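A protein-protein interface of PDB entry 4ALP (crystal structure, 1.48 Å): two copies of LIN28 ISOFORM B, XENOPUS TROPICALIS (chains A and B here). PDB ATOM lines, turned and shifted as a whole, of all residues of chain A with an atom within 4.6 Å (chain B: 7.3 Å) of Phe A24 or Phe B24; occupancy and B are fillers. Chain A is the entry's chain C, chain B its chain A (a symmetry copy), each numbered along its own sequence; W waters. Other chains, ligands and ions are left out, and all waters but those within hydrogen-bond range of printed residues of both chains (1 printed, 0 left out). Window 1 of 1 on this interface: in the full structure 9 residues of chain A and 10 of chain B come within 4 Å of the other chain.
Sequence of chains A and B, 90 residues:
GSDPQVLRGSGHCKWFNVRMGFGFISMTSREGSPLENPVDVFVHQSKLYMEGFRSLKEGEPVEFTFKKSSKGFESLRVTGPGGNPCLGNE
Water W1 lies within hydrogen-bond range of the indole nitrogen of Trp A15 (2.9 Å), the side-chain amino group of Lys A14 (3.3 Å) and the backbone carbonyl oxygen of Lys B71 (3.3 Å).
O of Lys B71 sits close to NE1 of Trp A15 (3.5 Å).
Printed residues of chain B that touch a printed residue of chain A: Trp B15, Phe B22, Phe B24, Phe B42 and Lys B71. Hydrophobic or aromatic side chains of chain B within 4 Å of the printed part of chain A: Trp B15, Phe B22, Phe B24 and Phe B42. Of the 12 printed residues of chain A, 4 touch a printed residue of chain B.
Phe B22 touches its own counterpart, Phe A22. Phe A22 touches Phe B42, but with the chains exchanged Phe A42 does not touch Phe B22 (4.5 Å). Phe B24 touches its own counterpart, Phe A24. Phe A42 touches Trp B15, but with the chains exchanged Trp A15 does not touch Phe B42 (5.8 Å). 12 positions are printed for both chains. Of the 5 pairs that touch across the chains among the printed residues, 2 have their exchanged pair printed and touching as well.
O of Trp A15 is in hydrogen-bond range of SG of Cys A13 (3.6 Å). The backbone NH (N) of Lys A14 lies within hydrogen-bond range of the backbone carbonyl oxygen (O) of Phe A24. The backbone carbonyl oxygen of Trp B15 sits at hydrogen-bond distance from the side-chain sulfur of Cys B13. The backbone carbonyl oxygen of Trp B15 is in hydrogen-bond range of the backbone NH of Phe B24 (3.0 Å). The backbone carbonyl oxygen of Phe B22 is in hydrogen-bond range of the backbone NH of Asn B17, at 2.9 Å. The side-chain carboxylate of Glu B74 lies within salt-bridge range of the side-chain amino group of Lys B71 (3.4 Å).
Of the printed residues of chain A, Phe B42 touches Phe A22. Of the printed residues of chain A, Phe B22 touches Phe A22 (3.4 Å). Of the printed residues of chain A, Trp B15 touches Phe A42. Met B27 touches none of the printed residues of chain A. The nearest residue of chain B that does not touch Phe A24 is Trp B15 (5.4 Å). The nearest residue of chain A that does not touch Phe B24 is Phe A22 (4.03 Å). The nearest printed residue of chain A that does not touch Trp B15 is Phe A24 (5.4 Å).
Among the printed residues, merely in contact across the chains: Phe A22 with Phe B22, Phe A22 with Phe B42, Phe A24 with Phe B24 and Phe A42 with Trp B15.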
ATOM      1  N   CYS A  13      -7.995   9.728  15.307  1.00  0.00           N
ATOM      2  CA  CYS A  13      -7.050  10.764  14.944  1.00  0.00           C
ATOM      3  C   CYS A  13      -7.516  12.139  15.369  1.00  0.00           C
ATOM      4  O   CYS A  13      -8.628  12.569  14.993  1.00  0.00           O
ATOM      5  CB  CYS A  13      -6.778  10.719  13.458  1.00  0.00           C
ATOM      6  SG  CYS A  13      -5.658  11.990  12.868  1.00  0.00           S
ATOM      7  N   LYS A  14      -6.714  12.817  16.144  1.00  0.00           N
ATOM      8  CA  LYS A  14      -6.979  14.183  16.570  1.00  0.00           C
ATOM      9  C   LYS A  14      -6.692  15.149  15.422  1.00  0.00           C
ATOM     10  O   LYS A  14      -7.569  15.945  15.038  1.00  0.00           O
ATOM     11  CB  LYS A  14      -6.152  14.517  17.806  1.00  0.00           C
ATOM     12  CG  LYS A  14      -6.476  15.841  18.467  1.00  0.00           C
ATOM     13  CD  LYS A  14      -5.452  16.214  19.508  1.00  0.00           C
ATOM     14  CE  LYS A  14      -6.042  17.152  20.531  1.00  0.00           C
ATOM     15  NZ  LYS A  14      -4.952  17.659  21.403  1.00  0.00           N
ATOM     16  N   TRP A  15      -5.470  15.104  14.876  1.00  0.00           N
ATOM     17  CA  TRP A  15      -5.108  15.767  13.665  1.00  0.00           C
ATOM     18  C   TRP A  15      -3.879  15.105  13.106  1.00  0.00           C
ATOM     19  O   TRP A  15      -3.165  14.381  13.803  1.00  0.00           O
ATOM     20  CB  TRP A  15      -4.858  17.281  13.881  1.00  0.00           C
ATOM     21  CG  TRP A  15      -3.841  17.668  14.910  1.00  0.00           C
ATOM     22  CD1 TRP A  15      -4.095  18.048  16.214  1.00  0.00           C
ATOM     23  CD2 TRP A  15      -2.417  17.807  14.743  1.00  0.00           C
ATOM     24  NE1 TRP A  15      -2.951  18.360  16.867  1.00  0.00           N
ATOM     25  CE2 TRP A  15      -1.887  18.236  16.054  1.00  0.00           C
ATOM     26  CE3 TRP A  15      -1.536  17.601  13.703  1.00  0.00           C
ATOM     27  CZ2 TRP A  15      -0.550  18.482  16.235  1.00  0.00           C
ATOM     28  CZ3 TRP A  15      -0.171  17.825  13.906  1.00  0.00           C
ATOM     29  CH2 TRP A  15       0.300  18.279  15.149  1.00  0.00           C
ATOM     30  N   PHE A  22       3.204  13.314  10.408  1.00  0.00           N
ATOM     31  CA  PHE A  22       2.914  12.975  11.805  1.00  0.00           C
ATOM     32  C   PHE A  22       1.653  13.650  12.255  1.00  0.00           C
ATOM     33  O   PHE A  22       1.154  14.611  11.620  1.00  0.00           O
ATOM     34  CB  PHE A  22       4.047  13.363  12.732  1.00  0.00           C
ATOM     35  CG  PHE A  22       4.027  14.811  13.116  1.00  0.00           C
ATOM     36  CD1 PHE A  22       4.456  15.804  12.233  1.00  0.00           C
ATOM     37  CD2 PHE A  22       3.449  15.199  14.319  1.00  0.00           C
ATOM     38  CE1 PHE A  22       4.386  17.125  12.597  1.00  0.00           C
ATOM     39  CE2 PHE A  22       3.354  16.545  14.684  1.00  0.00           C
ATOM     40  CZ  PHE A  22       3.812  17.486  13.804  1.00  0.00           C
ATOM     41  N   GLY A  23       1.166  13.211  13.386  1.00  0.00           N
ATOM     42  CA  GLY A  23       0.018  13.810  14.040  1.00  0.00           C
ATOM     43  C   GLY A  23      -0.128  13.301  15.467  1.00  0.00           C
ATOM     44  O   GLY A  23       0.819  12.759  16.050  1.00  0.00           O
ATOM     45  N   PHE A  24      -1.338  13.418  15.962  1.00  0.00           N
ATOM     46  CA  PHE A  24      -1.713  12.934  17.270  1.00  0.00           C
ATOM     47  C   PHE A  24      -3.025  12.163  17.157  1.00  0.00           C
ATOM     48  O   PHE A  24      -3.916  12.490  16.361  1.00  0.00           O
ATOM     49  CB  PHE A  24      -1.844  14.031  18.306  1.00  0.00           C
ATOM     50  CG  PHE A  24      -0.529  14.585  18.734  1.00  0.00           C
ATOM     51  CD1 PHE A  24       0.086  15.562  17.982  1.00  0.00           C
ATOM     52  CD2 PHE A  24       0.173  14.036  19.815  1.00  0.00           C
ATOM     53  CE1 PHE A  24       1.335  16.060  18.338  1.00  0.00           C
ATOM     54  CE2 PHE A  24       1.412  14.540  20.174  1.00  0.00           C
ATOM     55  CZ  PHE A  24       2.004  15.546  19.418  1.00  0.00           C
ATOM     56  N   ILE A  25      -3.111  11.132  17.971  1.00  0.00           N
ATOM     57  CA  ILE A  25      -4.298  10.346  18.232  1.00  0.00           C
ATOM     58  C   ILE A  25      -4.831  10.784  19.586  1.00  0.00           C
ATOM     59  O   ILE A  25      -4.087  11.011  20.516  1.00  0.00           O
ATOM     60  CB  ILE A  25      -3.976   8.836  18.269  1.00  0.00           C
ATOM     61  CG1 ILE A  25      -3.583   8.316  16.886  1.00  0.00           C
ATOM     62  CG2 ILE A  25      -5.088   8.028  18.919  1.00  0.00           C
ATOM     63  CD1 ILE A  25      -2.772   7.003  16.930  1.00  0.00           C
ATOM     64  N   SER A  26      -6.140  10.971  19.648  1.00  0.00           N
ATOM     65  CA  SER A  26      -6.830  11.158  20.891  1.00  0.00           C
ATOM     66  C   SER A  26      -7.211   9.763  21.376  1.00  0.00           C
ATOM     67  O   SER A  26      -8.139   9.125  20.845  1.00  0.00           O
ATOM     68  CB  SER A  26      -8.076  12.020  20.668  1.00  0.00           C
ATOM     69  OG  SER A  26      -8.717  12.360  21.893  1.00  0.00           O
ATOM     70  N   ASP A  40      -3.487  12.532  24.448  1.00  0.00           N
ATOM     71  CA  ASP A  40      -2.732  12.657  23.176  1.00  0.00           C
ATOM     72  C   ASP A  40      -1.647  11.614  23.047  1.00  0.00           C
ATOM     73  O   ASP A  40      -0.858  11.366  23.971  1.00  0.00           O
ATOM     74  CB  ASP A  40      -2.045  14.010  23.078  1.00  0.00           C
ATOM     75  CG  ASP A  40      -2.993  15.169  22.982  1.00  0.00           C
ATOM     76  OD1 ASP A  40      -4.158  15.023  22.591  1.00  0.00           O
ATOM     77  OD2 ASP A  40      -2.519  16.278  23.325  1.00  0.00           O
ATOM     78  N   VAL A  41      -1.595  10.958  21.890  1.00  0.00           N
ATOM     79  CA  VAL A  41      -0.553   9.983  21.593  1.00  0.00           C
ATOM     80  C   VAL A  41       0.029  10.402  20.241  1.00  0.00           C
ATOM     81  O   VAL A  41      -0.679  10.466  19.223  1.00  0.00           O
ATOM     82  CB  VAL A  41      -1.109   8.548  21.502  1.00  0.00           C
ATOM     83  CG1 VAL A  41      -0.024   7.529  21.221  1.00  0.00           C
ATOM     84  CG2 VAL A  41      -1.836   8.190  22.795  1.00  0.00           C
ATOM     85  N   PHE A  42       1.303  10.713  20.234  1.00  0.00           N
ATOM     86  CA  PHE A  42       1.999  11.042  18.980  1.00  0.00           C
ATOM     87  C   PHE A  42       1.943   9.861  18.023  1.00  0.00           C
ATOM     88  O   PHE A  42       2.063   8.696  18.425  1.00  0.00           O
ATOM     89  CB  PHE A  42       3.458  11.337  19.311  1.00  0.00           C
ATOM     90  CG  PHE A  42       4.314  11.624  18.123  1.00  0.00           C
ATOM     91  CD1 PHE A  42       4.400  12.908  17.570  1.00  0.00           C
ATOM     92  CD2 PHE A  42       5.074  10.617  17.559  1.00  0.00           C
ATOM     93  CE1 PHE A  42       5.246  13.145  16.480  1.00  0.00           C
ATOM     94  CE2 PHE A  42       5.902  10.873  16.477  1.00  0.00           C
ATOM     95  CZ  PHE A  42       5.965  12.140  15.940  1.00  0.00           C
ATOM     96  N   VAL A  43       1.813  10.154  16.728  1.00  0.00           N
ATOM     97  CA  VAL A  43       1.849   9.105  15.702  1.00  0.00           C
ATOM     98  C   VAL A  43       2.625   9.562  14.455  1.00  0.00           C
ATOM     99  O   VAL A  43       2.367  10.632  13.925  1.00  0.00           O
ATOM    100  CB  VAL A  43       0.439   8.660  15.299  1.00  0.00           C
ATOM    101  CG1 VAL A  43      -0.430   9.832  14.904  1.00  0.00           C
ATOM    102  CG2 VAL A  43       0.528   7.609  14.185  1.00  0.00           C
ATOM    103  N   HIS B  12      11.109  25.434  27.192  1.00  0.00           N
ATOM    104  CA  HIS B  12      12.198  24.511  26.925  1.00  0.00           C
ATOM    105  C   HIS B  12      11.794  23.443  25.948  1.00  0.00           C
ATOM    106  O   HIS B  12      10.622  23.223  25.746  1.00  0.00           O
ATOM    107  CB  HIS B  12      12.669  23.855  28.238  1.00  0.00           C
ATOM    108  CG  HIS B  12      11.629  23.062  28.904  1.00  0.00           C
ATOM    109  ND1 HIS B  12      10.749  23.578  29.810  1.00  0.00           N
ATOM    110  CD2 HIS B  12      11.281  21.724  28.735  1.00  0.00           C
ATOM    111  CE1 HIS B  12       9.914  22.594  30.205  1.00  0.00           C
ATOM    112  NE2 HIS B  12      10.215  21.482  29.541  1.00  0.00           N
ATOM    113  N   CYS B  13      12.765  22.878  25.266  1.00  0.00           N
ATOM    114  CA  CYS B  13      12.482  21.777  24.340  1.00  0.00           C
ATOM    115  C   CYS B  13      11.939  20.568  25.100  1.00  0.00           C
ATOM    116  O   CYS B  13      12.603  20.035  25.999  1.00  0.00           O
ATOM    117  CB  CYS B  13      13.759  21.431  23.579  1.00  0.00           C
ATOM    118  SG  CYS B  13      13.603  20.015  22.489  1.00  0.00           S
ATOM    119  N   LYS B  14      10.782  20.111  24.702  1.00  0.00           N
ATOM    120  CA  LYS B  14      10.212  18.836  25.132  1.00  0.00           C
ATOM    121  C   LYS B  14      10.915  17.661  24.476  1.00  0.00           C
ATOM    122  O   LYS B  14      11.431  16.784  25.160  1.00  0.00           O
ATOM    123  CB  LYS B  14       8.694  18.802  24.901  1.00  0.00           C
ATOM    124  CG  LYS B  14       8.032  17.605  25.491  1.00  0.00           C
ATOM    125  CD  LYS B  14       6.561  17.575  25.126  1.00  0.00           C
ATOM    126  CE  LYS B  14       5.864  16.459  25.824  1.00  0.00           C
ATOM    127  NZ  LYS B  14       4.460  16.330  25.327  1.00  0.00           N
ATOM    128  N   TRP B  15      10.961  17.651  23.150  1.00  0.00           N
ATOM    129  CA  TRP B  15      11.696  16.680  22.371  1.00  0.00           C
ATOM    130  C   TRP B  15      11.997  17.262  21.029  1.00  0.00           C
ATOM    131  O   TRP B  15      11.328  18.180  20.556  1.00  0.00           O
ATOM    132  CB  TRP B  15      10.920  15.371  22.216  1.00  0.00           C
ATOM    133  CG  TRP B  15       9.625  15.455  21.519  1.00  0.00           C
ATOM    134  CD1 TRP B  15       8.388  15.726  22.071  1.00  0.00           C
ATOM    135  CD2 TRP B  15       9.387  15.204  20.107  1.00  0.00           C
ATOM    136  NE1 TRP B  15       7.408  15.691  21.082  1.00  0.00           N
ATOM    137  CE2 TRP B  15       7.958  15.384  19.893  1.00  0.00           C
ATOM    138  CE3 TRP B  15      10.189  14.830  19.032  1.00  0.00           C
ATOM    139  CZ2 TRP B  15       7.365  15.193  18.641  1.00  0.00           C
ATOM    140  CZ3 TRP B  15       9.595  14.678  17.779  1.00  0.00           C
ATOM    141  CH2 TRP B  15       8.230  14.851  17.596  1.00  0.00           C
ATOM    142  N   PHE B  16      13.026  16.736  20.400  1.00  0.00           N
ATOM    143  CA  PHE B  16      13.341  17.115  19.037  1.00  0.00           C
ATOM    144  C   PHE B  16      14.021  15.966  18.329  1.00  0.00           C
ATOM    145  O   PHE B  16      15.050  15.493  18.783  1.00  0.00           O
ATOM    146  CB  PHE B  16      14.226  18.372  19.028  1.00  0.00           C
ATOM    147  CG  PHE B  16      14.341  19.008  17.674  1.00  0.00           C
ATOM    148  CD1 PHE B  16      15.263  18.554  16.739  1.00  0.00           C
ATOM    149  CD2 PHE B  16      13.432  19.967  17.297  1.00  0.00           C
ATOM    150  CE1 PHE B  16      15.290  19.128  15.456  1.00  0.00           C
ATOM    151  CE2 PHE B  16      13.461  20.520  16.009  1.00  0.00           C
ATOM    152  CZ  PHE B  16      14.372  20.100  15.112  1.00  0.00           C
ATOM    153  N   ASN B  17      13.418  15.464  17.275  1.00  0.00           N
ATOM    154  CA  ASN B  17      13.936  14.317  16.551  1.00  0.00           C
ATOM    155  C   ASN B  17      14.598  14.798  15.274  1.00  0.00           C
ATOM    156  O   ASN B  17      13.964  15.362  14.408  1.00  0.00           O
ATOM    157  CB  ASN B  17      12.809  13.319  16.254  1.00  0.00           C
ATOM    158  CG  ASN B  17      13.292  12.099  15.556  1.00  0.00           C
ATOM    159  OD1 ASN B  17      13.857  12.151  14.473  1.00  0.00           O
ATOM    160  ND2 ASN B  17      13.082  10.947  16.192  1.00  0.00           N
ATOM    161  N   PHE B  22      11.930  17.822  13.416  1.00  0.00           N
ATOM    162  CA  PHE B  22      10.976  18.588  14.165  1.00  0.00           C
ATOM    163  C   PHE B  22      10.804  18.044  15.590  1.00  0.00           C
ATOM    164  O   PHE B  22      11.330  16.958  15.904  1.00  0.00           O
ATOM    165  CB  PHE B  22       9.642  18.752  13.438  1.00  0.00           C
ATOM    166  CG  PHE B  22       8.988  17.461  13.021  1.00  0.00           C
ATOM    167  CD1 PHE B  22       8.396  16.612  13.933  1.00  0.00           C
ATOM    168  CD2 PHE B  22       8.956  17.115  11.671  1.00  0.00           C
ATOM    169  CE1 PHE B  22       7.799  15.430  13.538  1.00  0.00           C
ATOM    170  CE2 PHE B  22       8.364  15.939  11.268  1.00  0.00           C
ATOM    171  CZ  PHE B  22       7.804  15.096  12.199  1.00  0.00           C
ATOM    172  N   GLY B  23      10.041  18.758  16.391  1.00  0.00           N
ATOM    173  CA  GLY B  23       9.753  18.400  17.773  1.00  0.00           C
ATOM    174  C   GLY B  23       8.758  19.339  18.358  1.00  0.00           C
ATOM    175  O   GLY B  23       8.020  19.991  17.651  1.00  0.00           O
ATOM    176  N   PHE B  24       8.713  19.365  19.678  1.00  0.00           N
ATOM    177  CA  PHE B  24       7.860  20.278  20.439  1.00  0.00           C
ATOM    178  C   PHE B  24       8.611  20.992  21.533  1.00  0.00           C
ATOM    179  O   PHE B  24       9.532  20.430  22.132  1.00  0.00           O
ATOM    180  CB  PHE B  24       6.672  19.542  21.043  1.00  0.00           C
ATOM    181  CG  PHE B  24       5.572  19.314  20.056  1.00  0.00           C
ATOM    182  CD1 PHE B  24       5.621  18.260  19.124  1.00  0.00           C
ATOM    183  CD2 PHE B  24       4.511  20.196  19.977  1.00  0.00           C
ATOM    184  CE1 PHE B  24       4.630  18.100  18.173  1.00  0.00           C
ATOM    185  CE2 PHE B  24       3.535  20.010  19.017  1.00  0.00           C
ATOM    186  CZ  PHE B  24       3.595  18.974  18.113  1.00  0.00           C
ATOM    187  N   ILE B  25       8.215  22.230  21.754  1.00  0.00           N
ATOM    188  CA  ILE B  25       8.593  23.051  22.865  1.00  0.00           C
ATOM    189  C   ILE B  25       7.512  23.063  23.933  1.00  0.00           C
ATOM    190  O   ILE B  25       6.350  23.154  23.601  1.00  0.00           O
ATOM    191  CB  ILE B  25       8.846  24.495  22.394  1.00  0.00           C
ATOM    192  CG1 ILE B  25      10.061  24.500  21.455  1.00  0.00           C
ATOM    193  CG2 ILE B  25       8.954  25.469  23.579  1.00  0.00           C
ATOM    194  CD1 ILE B  25      10.234  25.768  20.650  1.00  0.00           C
ATOM    195  N   SER B  26       7.888  22.942  25.206  1.00  0.00           N
ATOM    196  CA  SER B  26       6.956  23.173  26.319  1.00  0.00           C
ATOM    197  C   SER B  26       7.060  24.667  26.661  1.00  0.00           C
ATOM    198  O   SER B  26       8.064  25.137  27.177  1.00  0.00           O
ATOM    199  CB  SER B  26       7.283  22.318  27.514  1.00  0.00           C
ATOM    200  OG  SER B  26       6.369  22.582  28.577  1.00  0.00           O
ATOM    201  N   MET B  27       6.010  25.417  26.333  1.00  0.00           N
ATOM    202  CA  MET B  27       5.952  26.851  26.641  1.00  0.00           C
ATOM    203  C   MET B  27       5.551  27.025  28.103  1.00  0.00           C
ATOM    204  O   MET B  27       4.454  26.632  28.498  1.00  0.00           O
ATOM    205  CB  MET B  27       4.930  27.556  25.752  1.00  0.00           C
ATOM    206  CG  MET B  27       4.767  29.039  26.074  1.00  0.00           C
ATOM    207  SD  MET B  27       3.888  29.983  24.814  1.00  0.00           S
ATOM    208  CE  MET B  27       2.378  29.033  24.553  1.00  0.00           C
ATOM    209  N   VAL B  39       2.117  24.797  27.755  1.00  0.00           N
ATOM    210  CA  VAL B  39       1.439  24.557  26.466  1.00  0.00           C
ATOM    211  C   VAL B  39       2.483  24.045  25.477  1.00  0.00           C
ATOM    212  O   VAL B  39       3.540  24.621  25.330  1.00  0.00           O
ATOM    213  CB  VAL B  39       0.817  25.850  25.954  1.00  0.00           C
ATOM    214  CG1 VAL B  39       0.274  25.690  24.523  1.00  0.00           C
ATOM    215  CG2 VAL B  39      -0.281  26.364  26.913  1.00  0.00           C
ATOM    216  N   ASP B  40       2.162  22.953  24.789  1.00  0.00           N
ATOM    217  CA  ASP B  40       3.098  22.442  23.760  1.00  0.00           C
ATOM    218  C   ASP B  40       2.991  23.259  22.475  1.00  0.00           C
ATOM    219  O   ASP B  40       1.891  23.606  22.054  1.00  0.00           O
ATOM    220  CB  ASP B  40       2.821  20.964  23.500  1.00  0.00           C
ATOM    221  CG  ASP B  40       3.377  20.055  24.631  1.00  0.00           C
ATOM    222  OD1 ASP B  40       4.149  20.531  25.499  1.00  0.00           O
ATOM    223  OD2 ASP B  40       3.116  18.822  24.609  1.00  0.00           O
ATOM    224  N   VAL B  41       4.133  23.579  21.883  1.00  0.00           N
ATOM    225  CA  VAL B  41       4.255  24.377  20.654  1.00  0.00           C
ATOM    226  C   VAL B  41       5.156  23.641  19.678  1.00  0.00           C
ATOM    227  O   VAL B  41       6.287  23.255  20.011  1.00  0.00           O
ATOM    228  CB  VAL B  41       4.854  25.761  20.978  1.00  0.00           C
ATOM    229  CG1 VAL B  41       5.006  26.608  19.715  1.00  0.00           C
ATOM    230  CG2 VAL B  41       4.026  26.479  22.046  1.00  0.00           C
ATOM    231  N   PHE B  42       4.664  23.372  18.481  1.00  0.00           N
ATOM    232  CA  PHE B  42       5.446  22.698  17.467  1.00  0.00           C
ATOM    233  C   PHE B  42       6.646  23.506  17.041  1.00  0.00           C
ATOM    234  O   PHE B  42       6.605  24.750  16.992  1.00  0.00           O
ATOM    235  CB  PHE B  42       4.547  22.435  16.260  1.00  0.00           C
ATOM    236  CG  PHE B  42       5.257  21.750  15.110  1.00  0.00           C
ATOM    237  CD1 PHE B  42       5.645  20.420  15.223  1.00  0.00           C
ATOM    238  CD2 PHE B  42       5.530  22.423  13.912  1.00  0.00           C
ATOM    239  CE1 PHE B  42       6.296  19.808  14.174  1.00  0.00           C
ATOM    240  CE2 PHE B  42       6.151  21.776  12.849  1.00  0.00           C
ATOM    241  CZ  PHE B  42       6.523  20.464  12.989  1.00  0.00           C
ATOM    242  N   VAL B  43       7.765  22.805  16.782  1.00  0.00           N
ATOM    243  CA  VAL B  43       8.950  23.492  16.274  1.00  0.00           C
ATOM    244  C   VAL B  43       9.568  22.645  15.154  1.00  0.00           C
ATOM    245  O   VAL B  43       9.882  21.445  15.321  1.00  0.00           O
ATOM    246  CB  VAL B  43       9.984  23.796  17.377  1.00  0.00           C
ATOM    247  CG1 VAL B  43      10.342  22.560  18.226  1.00  0.00           C
ATOM    248  CG2 VAL B  43      11.237  24.415  16.779  1.00  0.00           C
ATOM    249  N   HIS B  44       9.709  23.269  13.978  1.00  0.00           N
ATOM    250  CA  HIS B  44      10.424  22.680  12.851  1.00  0.00           C
ATOM    251  C   HIS B  44      11.826  23.185  12.789  1.00  0.00           C
ATOM    252  O   HIS B  44      12.114  24.334  13.127  1.00  0.00           O
ATOM    253  CB  HIS B  44       9.667  23.070  11.558  1.00  0.00           C
ATOM    254  CG  HIS B  44      10.119  22.308  10.371  1.00  0.00           C
ATOM    255  ND1 HIS B  44      10.954  22.821   9.425  1.00  0.00           N
ATOM    256  CD2 HIS B  44       9.849  21.016  10.003  1.00  0.00           C
ATOM    257  CE1 HIS B  44      11.210  21.889   8.524  1.00  0.00           C
ATOM    258  NE2 HIS B  44      10.574  20.766   8.873  1.00  0.00           N
ATOM    259  N   LEU B  56      17.500  21.067  18.486  1.00  0.00           N
ATOM    260  CA  LEU B  56      17.364  21.394  19.884  1.00  0.00           C
ATOM    261  C   LEU B  56      17.708  20.151  20.682  1.00  0.00           C
ATOM    262  O   LEU B  56      17.408  19.035  20.239  1.00  0.00           O
ATOM    263  CB  LEU B  56      15.939  21.838  20.226  1.00  0.00           C
ATOM    264  CG  LEU B  56      15.526  23.187  19.686  1.00  0.00           C
ATOM    265  CD1 LEU B  56      14.045  23.437  19.993  1.00  0.00           C
ATOM    266  CD2 LEU B  56      16.395  24.336  20.202  1.00  0.00           C
ATOM    267  N   LYS B  71      -2.458  22.714  14.144  1.00  0.00           N
ATOM    268  CA  LYS B  71      -1.615  21.885  15.019  1.00  0.00           C
ATOM    269  C   LYS B  71      -1.837  22.210  16.471  1.00  0.00           C
ATOM    270  O   LYS B  71      -1.432  21.438  17.357  1.00  0.00           O
ATOM    271  CB  LYS B  71      -0.131  22.049  14.738  1.00  0.00           C
ATOM    272  CG  LYS B  71       0.355  21.674  13.366  1.00  0.00           C
ATOM    273  CD  LYS B  71       1.890  21.719  13.305  1.00  0.00           C
ATOM    274  CE  LYS B  71       2.403  21.436  11.909  1.00  0.00           C
ATOM    275  NZ  LYS B  71       1.825  22.358  10.881  1.00  0.00           N
ATOM    276  N   GLY B  72      -2.502  23.309  16.815  1.00  0.00           N
ATOM    277  CA  GLY B  72      -2.470  23.749  18.198  1.00  0.00           C
ATOM    278  C   GLY B  72      -1.782  25.116  18.101  1.00  0.00           C
ATOM    279  O   GLY B  72      -2.438  26.126  17.800  1.00  0.00           O
ATOM    280  N   PHE B  73      -0.468  25.126  18.350  1.00  0.00           N
ATOM    281  CA  PHE B  73       0.410  26.271  18.252  1.00  0.00           C
ATOM    282  C   PHE B  73       1.712  25.859  17.600  1.00  0.00           C
ATOM    283  O   PHE B  73       2.156  24.701  17.786  1.00  0.00           O
ATOM    284  CB  PHE B  73       0.701  26.834  19.630  1.00  0.00           C
ATOM    285  CG  PHE B  73      -0.497  27.360  20.308  1.00  0.00           C
ATOM    286  CD1 PHE B  73      -1.003  28.602  19.955  1.00  0.00           C
ATOM    287  CD2 PHE B  73      -1.174  26.586  21.249  1.00  0.00           C
ATOM    288  CE1 PHE B  73      -2.186  29.080  20.549  1.00  0.00           C
ATOM    289  CE2 PHE B  73      -2.358  27.058  21.814  1.00  0.00           C
ATOM    290  CZ  PHE B  73      -2.833  28.297  21.489  1.00  0.00           C
ATOM    291  N   GLU B  74       2.261  26.735  16.772  1.00  0.00           N
ATOM    292  CA  GLU B  74       3.518  26.441  16.122  1.00  0.00           C
ATOM    293  C   GLU B  74       4.435  27.659  16.152  1.00  0.00           C
ATOM    294  O   GLU B  74       3.993  28.799  16.002  1.00  0.00           O
ATOM    295  CB  GLU B  74       3.342  25.943  14.698  1.00  0.00           C
ATOM    296  CG  GLU B  74       2.731  26.914  13.767  1.00  0.00           C
ATOM    297  CD  GLU B  74       2.545  26.269  12.383  1.00  0.00           C
ATOM    298  OE1 GLU B  74       1.587  25.484  12.247  1.00  0.00           O
ATOM    299  OE2 GLU B  74       3.419  26.501  11.512  1.00  0.00           O
HETATM  300  O   HOH W   1      -2.889  19.476  19.581  1.00  0.00           O
